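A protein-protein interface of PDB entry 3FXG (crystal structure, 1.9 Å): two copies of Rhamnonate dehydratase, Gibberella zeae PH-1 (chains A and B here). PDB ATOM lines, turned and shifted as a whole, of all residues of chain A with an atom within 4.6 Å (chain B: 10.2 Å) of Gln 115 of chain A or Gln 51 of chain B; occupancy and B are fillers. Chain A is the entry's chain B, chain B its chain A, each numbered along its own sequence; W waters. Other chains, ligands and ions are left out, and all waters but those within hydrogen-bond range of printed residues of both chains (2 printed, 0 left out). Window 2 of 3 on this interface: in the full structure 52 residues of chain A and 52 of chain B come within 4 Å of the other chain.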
ATOM      1  N   PHE A 100       9.070  -2.536   6.078  1.00  0.00           N
ATOM      2  CA  PHE A 100       8.110  -3.607   5.824  1.00  0.00           C
ATOM      3  C   PHE A 100       7.555  -4.230   7.101  1.00  0.00           C
ATOM      4  O   PHE A 100       6.477  -4.824   7.091  1.00  0.00           O
ATOM      5  CB  PHE A 100       8.776  -4.716   5.004  1.00  0.00           C
ATOM      6  CG  PHE A 100       9.393  -4.236   3.725  1.00  0.00           C
ATOM      7  CD1 PHE A 100       8.594  -3.862   2.652  1.00  0.00           C
ATOM      8  CD2 PHE A 100      10.775  -4.131   3.604  1.00  0.00           C
ATOM      9  CE1 PHE A 100       9.162  -3.386   1.472  1.00  0.00           C
ATOM     10  CE2 PHE A 100      11.352  -3.655   2.429  1.00  0.00           C
ATOM     11  CZ  PHE A 100      10.543  -3.283   1.362  1.00  0.00           C
ATOM     12  N   LEU A 111       4.181 -13.089   3.447  1.00  0.00           N
ATOM     13  CA  LEU A 111       4.170 -11.753   2.862  1.00  0.00           C
ATOM     14  C   LEU A 111       5.468 -11.005   3.152  1.00  0.00           C
ATOM     15  O   LEU A 111       6.111 -10.482   2.245  1.00  0.00           O
ATOM     16  CB  LEU A 111       2.998 -10.940   3.418  1.00  0.00           C
ATOM     17  CG  LEU A 111       2.939  -9.470   2.984  1.00  0.00           C
ATOM     18  CD1 LEU A 111       2.708  -9.387   1.487  1.00  0.00           C
ATOM     19  CD2 LEU A 111       1.824  -8.752   3.732  1.00  0.00           C
ATOM     20  N   LEU A 112       5.844 -10.959   4.425  1.00  0.00           N
ATOM     21  CA  LEU A 112       7.043 -10.245   4.827  1.00  0.00           C
ATOM     22  C   LEU A 112       8.289 -10.754   4.118  1.00  0.00           C
ATOM     23  O   LEU A 112       9.141  -9.960   3.716  1.00  0.00           O
ATOM     24  CB  LEU A 112       7.211 -10.313   6.348  1.00  0.00           C
ATOM     25  CG  LEU A 112       6.083  -9.634   7.139  1.00  0.00           C
ATOM     26  CD1 LEU A 112       6.357  -9.749   8.629  1.00  0.00           C
ATOM     27  CD2 LEU A 112       5.964  -8.167   6.733  1.00  0.00           C
ATOM     28  N   PHE A 113       8.407 -12.070   3.957  1.00  0.00           N
ATOM     29  CA  PHE A 113       9.572 -12.600   3.267  1.00  0.00           C
ATOM     30  C   PHE A 113       9.582 -12.194   1.795  1.00  0.00           C
ATOM     31  O   PHE A 113      10.604 -11.750   1.282  1.00  0.00           O
ATOM     32  CB  PHE A 113       9.644 -14.126   3.342  1.00  0.00           C
ATOM     33  CG  PHE A 113      10.788 -14.691   2.555  1.00  0.00           C
ATOM     34  CD1 PHE A 113      12.081 -14.671   3.072  1.00  0.00           C
ATOM     35  CD2 PHE A 113      10.593 -15.148   1.254  1.00  0.00           C
ATOM     36  CE1 PHE A 113      13.167 -15.095   2.298  1.00  0.00           C
ATOM     37  CE2 PHE A 113      11.668 -15.571   0.474  1.00  0.00           C
ATOM     38  CZ  PHE A 113      12.956 -15.543   0.997  1.00  0.00           C
ATOM     39  N   GLU A 114       8.451 -12.355   1.112  1.00  0.00           N
ATOM     40  CA  GLU A 114       8.389 -12.000  -0.305  1.00  0.00           C
ATOM     41  C   GLU A 114       8.703 -10.518  -0.525  1.00  0.00           C
ATOM     42  O   GLU A 114       9.389 -10.160  -1.483  1.00  0.00           O
ATOM     43  CB  GLU A 114       7.009 -12.324  -0.893  1.00  0.00           C
ATOM     44  CG  GLU A 114       6.637 -13.808  -0.896  1.00  0.00           C
ATOM     45  CD  GLU A 114       7.625 -14.674  -1.665  1.00  0.00           C
ATOM     46  OE1 GLU A 114       7.882 -14.383  -2.849  1.00  0.00           O
ATOM     47  OE2 GLU A 114       8.138 -15.653  -1.081  1.00  0.00           O
ATOM     48  N   GLN A 115       8.208  -9.656   0.358  1.00  0.00           N
ATOM     49  CA  GLN A 115       8.470  -8.225   0.216  1.00  0.00           C
ATOM     50  C   GLN A 115       9.948  -7.906   0.447  1.00  0.00           C
ATOM     51  O   GLN A 115      10.561  -7.173  -0.330  1.00  0.00           O
ATOM     52  CB  GLN A 115       7.606  -7.412   1.190  1.00  0.00           C
ATOM     53  CG  GLN A 115       6.108  -7.559   0.953  1.00  0.00           C
ATOM     54  CD  GLN A 115       5.273  -6.635   1.825  1.00  0.00           C
ATOM     55  OE1 GLN A 115       5.566  -6.443   3.006  1.00  0.00           O
ATOM     56  NE2 GLN A 115       4.214  -6.070   1.246  1.00  0.00           N
ATOM     57  N   MET A 116      10.527  -8.452   1.509  1.00  0.00           N
ATOM     58  CA  MET A 116      11.934  -8.180   1.776  1.00  0.00           C
ATOM     59  C   MET A 116      12.811  -8.746   0.665  1.00  0.00           C
ATOM     60  O   MET A 116      13.767  -8.104   0.232  1.00  0.00           O
ATOM     61  CB  MET A 116      12.362  -8.774   3.122  1.00  0.00           C
ATOM     62  CG  MET A 116      11.720  -8.111   4.330  1.00  0.00           C
ATOM     63  SD  MET A 116      12.522  -8.687   6.001  1.00  0.00           S
ATOM     64  CE  MET A 116      11.531 -10.334   6.258  1.00  0.00           C
ATOM     65  N   TYR A 117      12.480  -9.942   0.188  1.00  0.00           N
ATOM     66  CA  TYR A 117      13.288 -10.562  -0.861  1.00  0.00           C
ATOM     67  C   TYR A 117      13.188  -9.841  -2.201  1.00  0.00           C
ATOM     68  O   TYR A 117      14.204  -9.508  -2.813  1.00  0.00           O
ATOM     69  CB  TYR A 117      12.894 -12.026  -1.061  1.00  0.00           C
ATOM     70  CG  TYR A 117      13.807 -12.763  -2.022  1.00  0.00           C
ATOM     71  CD1 TYR A 117      15.010 -13.320  -1.585  1.00  0.00           C
ATOM     72  CD2 TYR A 117      13.488 -12.867  -3.374  1.00  0.00           C
ATOM     73  CE1 TYR A 117      15.877 -13.968  -2.476  1.00  0.00           C
ATOM     74  CE2 TYR A 117      14.347 -13.506  -4.274  1.00  0.00           C
ATOM     75  CZ  TYR A 117      15.537 -14.055  -3.818  1.00  0.00           C
ATOM     76  OH  TYR A 117      16.380 -14.692  -4.709  1.00  0.00           O
ATOM     77  N   ARG A 118      11.966  -9.601  -2.662  1.00  0.00           N
ATOM     78  CA  ARG A 118      11.788  -8.947  -3.946  1.00  0.00           C
ATOM     79  C   ARG A 118      12.206  -7.479  -3.948  1.00  0.00           C
ATOM     80  O   ARG A 118      12.664  -6.969  -4.968  1.00  0.00           O
ATOM     81  CB  ARG A 118      10.339  -9.115  -4.426  1.00  0.00           C
ATOM     82  CG  ARG A 118      10.033 -10.561  -4.827  1.00  0.00           C
ATOM     83  CD  ARG A 118       8.601 -10.762  -5.300  1.00  0.00           C
ATOM     84  NE  ARG A 118       8.337 -10.202  -6.624  1.00  0.00           N
ATOM     85  CZ  ARG A 118       8.721 -10.753  -7.773  1.00  0.00           C
ATOM     86  NH1 ARG A 118       9.406 -11.892  -7.777  1.00  0.00           N
ATOM     87  NH2 ARG A 118       8.387 -10.181  -8.928  1.00  0.00           N
ATOM     88  N   ALA A 119      12.075  -6.808  -2.808  1.00  0.00           N
ATOM     89  CA  ALA A 119      12.458  -5.402  -2.718  1.00  0.00           C
ATOM     90  C   ALA A 119      13.977  -5.221  -2.713  1.00  0.00           C
ATOM     91  O   ALA A 119      14.476  -4.145  -3.046  1.00  0.00           O
ATOM     92  CB  ALA A 119      11.850  -4.768  -1.457  1.00  0.00           C
ATOM     93  N   ILE B  38      12.039   7.217 -10.592  1.00  0.00           N
ATOM     94  CA  ILE B  38      11.438   6.761  -9.345  1.00  0.00           C
ATOM     95  C   ILE B  38       9.965   7.117  -9.154  1.00  0.00           C
ATOM     96  O   ILE B  38       9.283   6.487  -8.346  1.00  0.00           O
ATOM     97  CB  ILE B  38      12.211   7.316  -8.127  1.00  0.00           C
ATOM     98  CG1 ILE B  38      12.217   8.848  -8.174  1.00  0.00           C
ATOM     99  CG2 ILE B  38      13.634   6.774  -8.117  1.00  0.00           C
ATOM    100  CD1 ILE B  38      12.886   9.504  -6.976  1.00  0.00           C
ATOM    101  N   THR B  44       7.689  -3.236 -11.365  1.00  0.00           N
ATOM    102  CA  THR B  44       8.850  -3.737 -10.631  1.00  0.00           C
ATOM    103  C   THR B  44       8.465  -4.993  -9.843  1.00  0.00           C
ATOM    104  O   THR B  44       7.290  -5.363  -9.788  1.00  0.00           O
ATOM    105  CB  THR B  44       9.377  -2.689  -9.621  1.00  0.00           C
ATOM    106  OG1 THR B  44       8.546  -2.691  -8.455  1.00  0.00           O
ATOM    107  CG2 THR B  44       9.370  -1.289 -10.235  1.00  0.00           C
ATOM    108  N   PRO B  45       9.455  -5.670  -9.231  1.00  0.00           N
ATOM    109  CA  PRO B  45       9.187  -6.882  -8.448  1.00  0.00           C
ATOM    110  C   PRO B  45       8.283  -6.603  -7.244  1.00  0.00           C
ATOM    111  O   PRO B  45       7.654  -7.515  -6.709  1.00  0.00           O
ATOM    112  CB  PRO B  45      10.582  -7.331  -8.012  1.00  0.00           C
ATOM    113  CG  PRO B  45      11.447  -6.874  -9.143  1.00  0.00           C
ATOM    114  CD  PRO B  45      10.907  -5.483  -9.411  1.00  0.00           C
ATOM    115  N   ALA B  46       8.227  -5.341  -6.824  1.00  0.00           N
ATOM    116  CA  ALA B  46       7.409  -4.951  -5.677  1.00  0.00           C
ATOM    117  C   ALA B  46       6.054  -4.365  -6.069  1.00  0.00           C
ATOM    118  O   ALA B  46       5.252  -4.017  -5.204  1.00  0.00           O
ATOM    119  CB  ALA B  46       8.173  -3.951  -4.813  1.00  0.00           C
ATOM    120  N   SER B  47       5.794  -4.259  -7.369  1.00  0.00           N
ATOM    121  CA  SER B  47       4.530  -3.700  -7.843  1.00  0.00           C
ATOM    122  C   SER B  47       3.324  -4.540  -7.439  1.00  0.00           C
ATOM    123  O   SER B  47       2.180  -4.114  -7.602  1.00  0.00           O
ATOM    124  CB  SER B  47       4.564  -3.538  -9.365  1.00  0.00           C
ATOM    125  OG  SER B  47       5.515  -2.558  -9.740  1.00  0.00           O
ATOM    126  N   LYS B  48       3.587  -5.732  -6.913  1.00  0.00           N
ATOM    127  CA  LYS B  48       2.534  -6.640  -6.470  1.00  0.00           C
ATOM    128  C   LYS B  48       1.755  -6.032  -5.300  1.00  0.00           C
ATOM    129  O   LYS B  48       0.601  -6.390  -5.058  1.00  0.00           O
ATOM    130  CB  LYS B  48       3.147  -7.974  -6.023  1.00  0.00           C
ATOM    131  CG  LYS B  48       4.078  -8.621  -7.048  1.00  0.00           C
ATOM    132  CD  LYS B  48       4.807  -9.833  -6.468  1.00  0.00           C
ATOM    133  CE  LYS B  48       3.854 -10.949  -6.065  1.00  0.00           C
ATOM    134  NZ  LYS B  48       3.152 -11.560  -7.232  1.00  0.00           N
ATOM    135  N   TRP B  49       2.385  -5.104  -4.587  1.00  0.00           N
ATOM    136  CA  TRP B  49       1.761  -4.477  -3.426  1.00  0.00           C
ATOM    137  C   TRP B  49       1.470  -2.987  -3.621  1.00  0.00           C
ATOM    138  O   TRP B  49       2.359  -2.201  -3.947  1.00  0.00           O
ATOM    139  CB  TRP B  49       2.661  -4.709  -2.210  1.00  0.00           C
ATOM    140  CG  TRP B  49       3.014  -6.163  -2.054  1.00  0.00           C
ATOM    141  CD1 TRP B  49       2.162  -7.181  -1.727  1.00  0.00           C
ATOM    142  CD2 TRP B  49       4.293  -6.772  -2.288  1.00  0.00           C
ATOM    143  NE1 TRP B  49       2.829  -8.384  -1.747  1.00  0.00           N
ATOM    144  CE2 TRP B  49       4.138  -8.161  -2.086  1.00  0.00           C
ATOM    145  CE3 TRP B  49       5.556  -6.276  -2.650  1.00  0.00           C
ATOM    146  CZ2 TRP B  49       5.199  -9.068  -2.235  1.00  0.00           C
ATOM    147  CZ3 TRP B  49       6.614  -7.179  -2.799  1.00  0.00           C
ATOM    148  CH2 TRP B  49       6.425  -8.559  -2.590  1.00  0.00           C
ATOM    149  N   GLU B  50       0.209  -2.615  -3.412  1.00  0.00           N
ATOM    150  CA  GLU B  50      -0.252  -1.238  -3.580  1.00  0.00           C
ATOM    151  C   GLU B  50       0.628  -0.133  -3.005  1.00  0.00           C
ATOM    152  O   GLU B  50       0.942   0.837  -3.697  1.00  0.00           O
ATOM    153  CB  GLU B  50      -1.670  -1.094  -3.015  1.00  0.00           C
ATOM    154  CG  GLU B  50      -2.750  -1.633  -3.937  1.00  0.00           C
ATOM    155  CD  GLU B  50      -2.916  -0.792  -5.191  1.00  0.00           C
ATOM    156  OE1 GLU B  50      -3.622  -1.240  -6.122  1.00  0.00           O
ATOM    157  OE2 GLU B  50      -2.347   0.320  -5.244  1.00  0.00           O
ATOM    158  N   GLN B  51       1.025  -0.267  -1.745  1.00  0.00           N
ATOM    159  CA  GLN B  51       1.845   0.762  -1.122  1.00  0.00           C
ATOM    160  C   GLN B  51       3.237   0.897  -1.738  1.00  0.00           C
ATOM    161  O   GLN B  51       3.955   1.849  -1.446  1.00  0.00           O
ATOM    162  CB  GLN B  51       1.962   0.524   0.391  1.00  0.00           C
ATOM    163  CG  GLN B  51       2.762  -0.703   0.822  1.00  0.00           C
ATOM    164  CD  GLN B  51       1.944  -1.986   0.865  1.00  0.00           C
ATOM    165  OE1 GLN B  51       2.209  -2.871   1.681  1.00  0.00           O
ATOM    166  NE2 GLN B  51       0.957  -2.099  -0.015  1.00  0.00           N
ATOM    167  N   TYR B  52       3.612  -0.041  -2.603  1.00  0.00           N
ATOM    168  CA  TYR B  52       4.930   0.011  -3.223  1.00  0.00           C
ATOM    169  C   TYR B  52       4.912   0.107  -4.744  1.00  0.00           C
ATOM    170  O   TYR B  52       5.957  -0.008  -5.378  1.00  0.00           O
ATOM    171  CB  TYR B  52       5.752  -1.214  -2.811  1.00  0.00           C
ATOM    172  CG  TYR B  52       5.974  -1.307  -1.321  1.00  0.00           C
ATOM    173  CD1 TYR B  52       6.643  -0.292  -0.636  1.00  0.00           C
ATOM    174  CD2 TYR B  52       5.482  -2.389  -0.587  1.00  0.00           C
ATOM    175  CE1 TYR B  52       6.814  -0.344   0.741  1.00  0.00           C
ATOM    176  CE2 TYR B  52       5.647  -2.452   0.798  1.00  0.00           C
ATOM    177  CZ  TYR B  52       6.314  -1.423   1.454  1.00  0.00           C
ATOM    178  OH  TYR B  52       6.466  -1.452   2.823  1.00  0.00           O
ATOM    179  N   LYS B  53       3.747   0.340  -5.339  1.00  0.00           N
ATOM    180  CA  LYS B  53       3.696   0.402  -6.794  1.00  0.00           C
ATOM    181  C   LYS B  53       3.783   1.779  -7.451  1.00  0.00           C
ATOM    182  O   LYS B  53       4.114   1.873  -8.629  1.00  0.00           O
ATOM    183  CB  LYS B  53       2.462  -0.353  -7.305  1.00  0.00           C
ATOM    184  CG  LYS B  53       1.135   0.154  -6.799  1.00  0.00           C
ATOM    185  CD  LYS B  53       0.028  -0.875  -7.035  1.00  0.00           C
ATOM    186  CE  LYS B  53      -0.082  -1.275  -8.499  1.00  0.00           C
ATOM    187  NZ  LYS B  53      -0.345  -0.099  -9.366  1.00  0.00           N
ATOM    188  N   LYS B  54       3.518   2.849  -6.707  1.00  0.00           N
ATOM    189  CA  LYS B  54       3.572   4.187  -7.296  1.00  0.00           C
ATOM    190  C   LYS B  54       4.964   4.820  -7.282  1.00  0.00           C
ATOM    191  O   LYS B  54       5.282   5.660  -8.124  1.00  0.00           O
ATOM    192  CB  LYS B  54       2.591   5.124  -6.583  1.00  0.00           C
ATOM    193  CG  LYS B  54       2.410   6.461  -7.289  1.00  0.00           C
ATOM    194  CD  LYS B  54       1.507   7.407  -6.507  1.00  0.00           C
ATOM    195  CE  LYS B  54       1.225   8.677  -7.299  1.00  0.00           C
ATOM    196  NZ  LYS B  54       2.474   9.379  -7.721  1.00  0.00           N
ATOM    197  N   SER B  55       5.789   4.417  -6.325  1.00  0.00           N
ATOM    198  CA  SER B  55       7.138   4.957  -6.194  1.00  0.00           C
ATOM    199  C   SER B  55       8.164   3.845  -6.032  1.00  0.00           C
ATOM    200  O   SER B  55       7.940   2.901  -5.275  1.00  0.00           O
ATOM    201  CB  SER B  55       7.202   5.881  -4.975  1.00  0.00           C
ATOM    202  OG  SER B  55       8.537   6.074  -4.545  1.00  0.00           O
ATOM    203  N   ARG B  56       9.290   3.950  -6.730  1.00  0.00           N
ATOM    204  CA  ARG B  56      10.313   2.921  -6.599  1.00  0.00           C
ATOM    205  C   ARG B  56      11.120   3.137  -5.322  1.00  0.00           C
ATOM    206  O   ARG B  56      11.739   2.205  -4.803  1.00  0.00           O
ATOM    207  CB  ARG B  56      11.224   2.889  -7.834  1.00  0.00           C
ATOM    208  CG  ARG B  56      10.493   2.408  -9.088  1.00  0.00           C
ATOM    209  CD  ARG B  56      11.395   1.635 -10.051  1.00  0.00           C
ATOM    210  NE  ARG B  56      12.262   2.501 -10.844  1.00  0.00           N
ATOM    211  CZ  ARG B  56      13.071   2.065 -11.806  1.00  0.00           C
ATOM    212  NH1 ARG B  56      13.132   0.770 -12.094  1.00  0.00           N
ATOM    213  NH2 ARG B  56      13.815   2.925 -12.490  1.00  0.00           N
ATOM    214  N   THR B  57      11.101   4.363  -4.802  1.00  0.00           N
ATOM    215  CA  THR B  57      11.819   4.654  -3.567  1.00  0.00           C
ATOM    216  C   THR B  57      11.038   4.101  -2.375  1.00  0.00           C
ATOM    217  O   THR B  57      11.617   3.797  -1.331  1.00  0.00           O
ATOM    218  CB  THR B  57      12.037   6.176  -3.362  1.00  0.00           C
ATOM    219  OG1 THR B  57      10.777   6.857  -3.399  1.00  0.00           O
ATOM    220  CG2 THR B  57      12.952   6.733  -4.448  1.00  0.00           C
ATOM    221  N   SER B  58       9.724   3.954  -2.540  1.00  0.00           N
ATOM    222  CA  SER B  58       8.881   3.439  -1.466  1.00  0.00           C
ATOM    223  C   SER B  58       9.404   2.097  -0.956  1.00  0.00           C
ATOM    224  O   SER B  58       9.479   1.879   0.258  1.00  0.00           O
ATOM    225  CB  SER B  58       7.433   3.287  -1.942  1.00  0.00           C
ATOM    226  OG  SER B  58       7.314   2.291  -2.944  1.00  0.00           O
ATOM    227  N   TRP B  59       9.775   1.207  -1.874  1.00  0.00           N
ATOM    228  CA  TRP B  59      10.296  -0.094  -1.469  1.00  0.00           C
ATOM    229  C   TRP B  59      11.814  -0.119  -1.289  1.00  0.00           C
ATOM    230  O   TRP B  59      12.386  -1.153  -0.946  1.00  0.00           O
ATOM    231  CB  TRP B  59       9.846  -1.210  -2.431  1.00  0.00           C
ATOM    232  CG  TRP B  59      10.067  -0.963  -3.893  1.00  0.00           C
ATOM    233  CD1 TRP B  59       9.165  -0.450  -4.783  1.00  0.00           C
ATOM    234  CD2 TRP B  59      11.245  -1.273  -4.648  1.00  0.00           C
ATOM    235  NE1 TRP B  59       9.706  -0.427  -6.046  1.00  0.00           N
ATOM    236  CE2 TRP B  59      10.982  -0.925  -5.994  1.00  0.00           C
ATOM    237  CE3 TRP B  59      12.496  -1.810  -4.322  1.00  0.00           C
ATOM    238  CZ2 TRP B  59      11.926  -1.096  -7.013  1.00  0.00           C
ATOM    239  CZ3 TRP B  59      13.440  -1.984  -5.340  1.00  0.00           C
ATOM    240  CH2 TRP B  59      13.146  -1.626  -6.668  1.00  0.00           C
ATOM    241  N   GLY B  60      12.463   1.018  -1.533  1.00  0.00           N
ATOM    242  CA  GLY B  60      13.899   1.111  -1.314  1.00  0.00           C
ATOM    243  C   GLY B  60      14.909   1.053  -2.446  1.00  0.00           C
ATOM    244  O   GLY B  60      16.076   0.764  -2.193  1.00  0.00           O
ATOM    245  N   ILE B  61      14.507   1.345  -3.677  1.00  0.00           N
ATOM    246  CA  ILE B  61      15.461   1.287  -4.782  1.00  0.00           C
ATOM    247  C   ILE B  61      16.653   2.231  -4.566  1.00  0.00           C
ATOM    248  O   ILE B  61      17.722   2.043  -5.147  1.00  0.00           O
ATOM    249  CB  ILE B  61      14.781   1.635  -6.127  1.00  0.00           C
ATOM    250  CG1 ILE B  61      15.648   1.140  -7.288  1.00  0.00           C
ATOM    251  CG2 ILE B  61      14.575   3.150  -6.233  1.00  0.00           C
ATOM    252  CD1 ILE B  61      14.968   1.229  -8.647  1.00  0.00           C
HETATM  253  O   HOH W   1       1.551  -5.111   2.637  1.00  0.00           O
HETATM  254  O   HOH W   2       6.327  -8.111 -10.162  1.00  0.00           O
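The backbone carbonyl oxygen (O) of Pro 45 of chain B sits at hydrogen-bond distance from the guanidinium group (NE) of Arg 118 of chain A, 2.8 Å away.
Phe 100 of chain A touches Tyr 52 of chain B.
O of Trp 59 of chain B touches CZ of Phe 100 of chain A, 3.6 Å away.
Leu 111 of chain A touches Trp 49 of chain B (CD1 to NE1, 3.4 Å).
CH2 of Trp 49 of chain B touches O of Glu 114 of chain A, at 3.5 Å.
Gln 115 of chain A touches Trp 49 of chain B.
OE1 of Gln 51 of chain B touches NE2 of Gln 115 of chain A, 3.8 Å away.
Gln 115 of chain A touches Tyr 52 of chain B.
NE of Arg 118 of chain A touches CD of Lys 48 of chain B, 3.6 Å away.
Trp 59 of chain B touches Ala 119 of chain A.
Printed residues of chain B within 4 Å of Gln 115 of chain A: Trp 49, Gln 51 and Tyr 52.
Gln 51 of chain B touches just one residue of chain A: Gln 115.
Phe 100 of chain A touches just these residues of chain B: Tyr 52 (3.2 Å) and Trp 59 (3.6 Å).
Leu 111 of chain A touches one residue of chain B.
Of chain B, only Trp 59 (3.3 Å) comes within 4 Å of Ala 119 of chain A.
Of the printed residues of chain A, Trp 49 of chain B touches Leu 111, Glu 114 and Gln 115.
Printed residues of chain A within 4 Å of Tyr 52 of chain B: Phe 100 and Gln 115.
Printed residues of chain A within 4 Å of Trp 59 of chain B: Phe 100 and Ala 119.
Of the printed residues of chain B, Glu 114 of chain A touches Trp 49.
Gly 60 of chain B touches none of the printed residues of chain A.
Ile 61 of chain B touches none of the printed residues of chain A.
Of the 19 printed residues of chain B, 6 touch a printed residue of chain A.
Hydrophobic or aromatic side chains of chain B that line the printed part of chain A: Pro 45, Trp 49, Tyr 52 and Trp 59.
Printed residues of chain A that touch a printed residue of chain B: Phe 100, Leu 111, Glu 114, Gln 115, Arg 118 and Ala 119.
Hydrophobic or aromatic side chains of chain A within 4 Å of the printed part of chain B: Phe 100, Leu 111 and Ala 119.
Among the printed residues, no Asp or Glu carboxylate lies within 4 Å of a Lys or Arg side-chain nitrogen of the other chain.
No position is printed for both chains.
Water W1 bridges OE1 of Gln 51 of chain B (2.5 Å) and NE2 of Gln 115 of chain A (3.2 Å).
Water W2 lies within hydrogen-bond range of the backbone carbonyl oxygen (O) of Thr 44 of chain B (2.9 Å) and the guanidinium group (NH2) of Arg 118 of chain A (3.2 Å).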
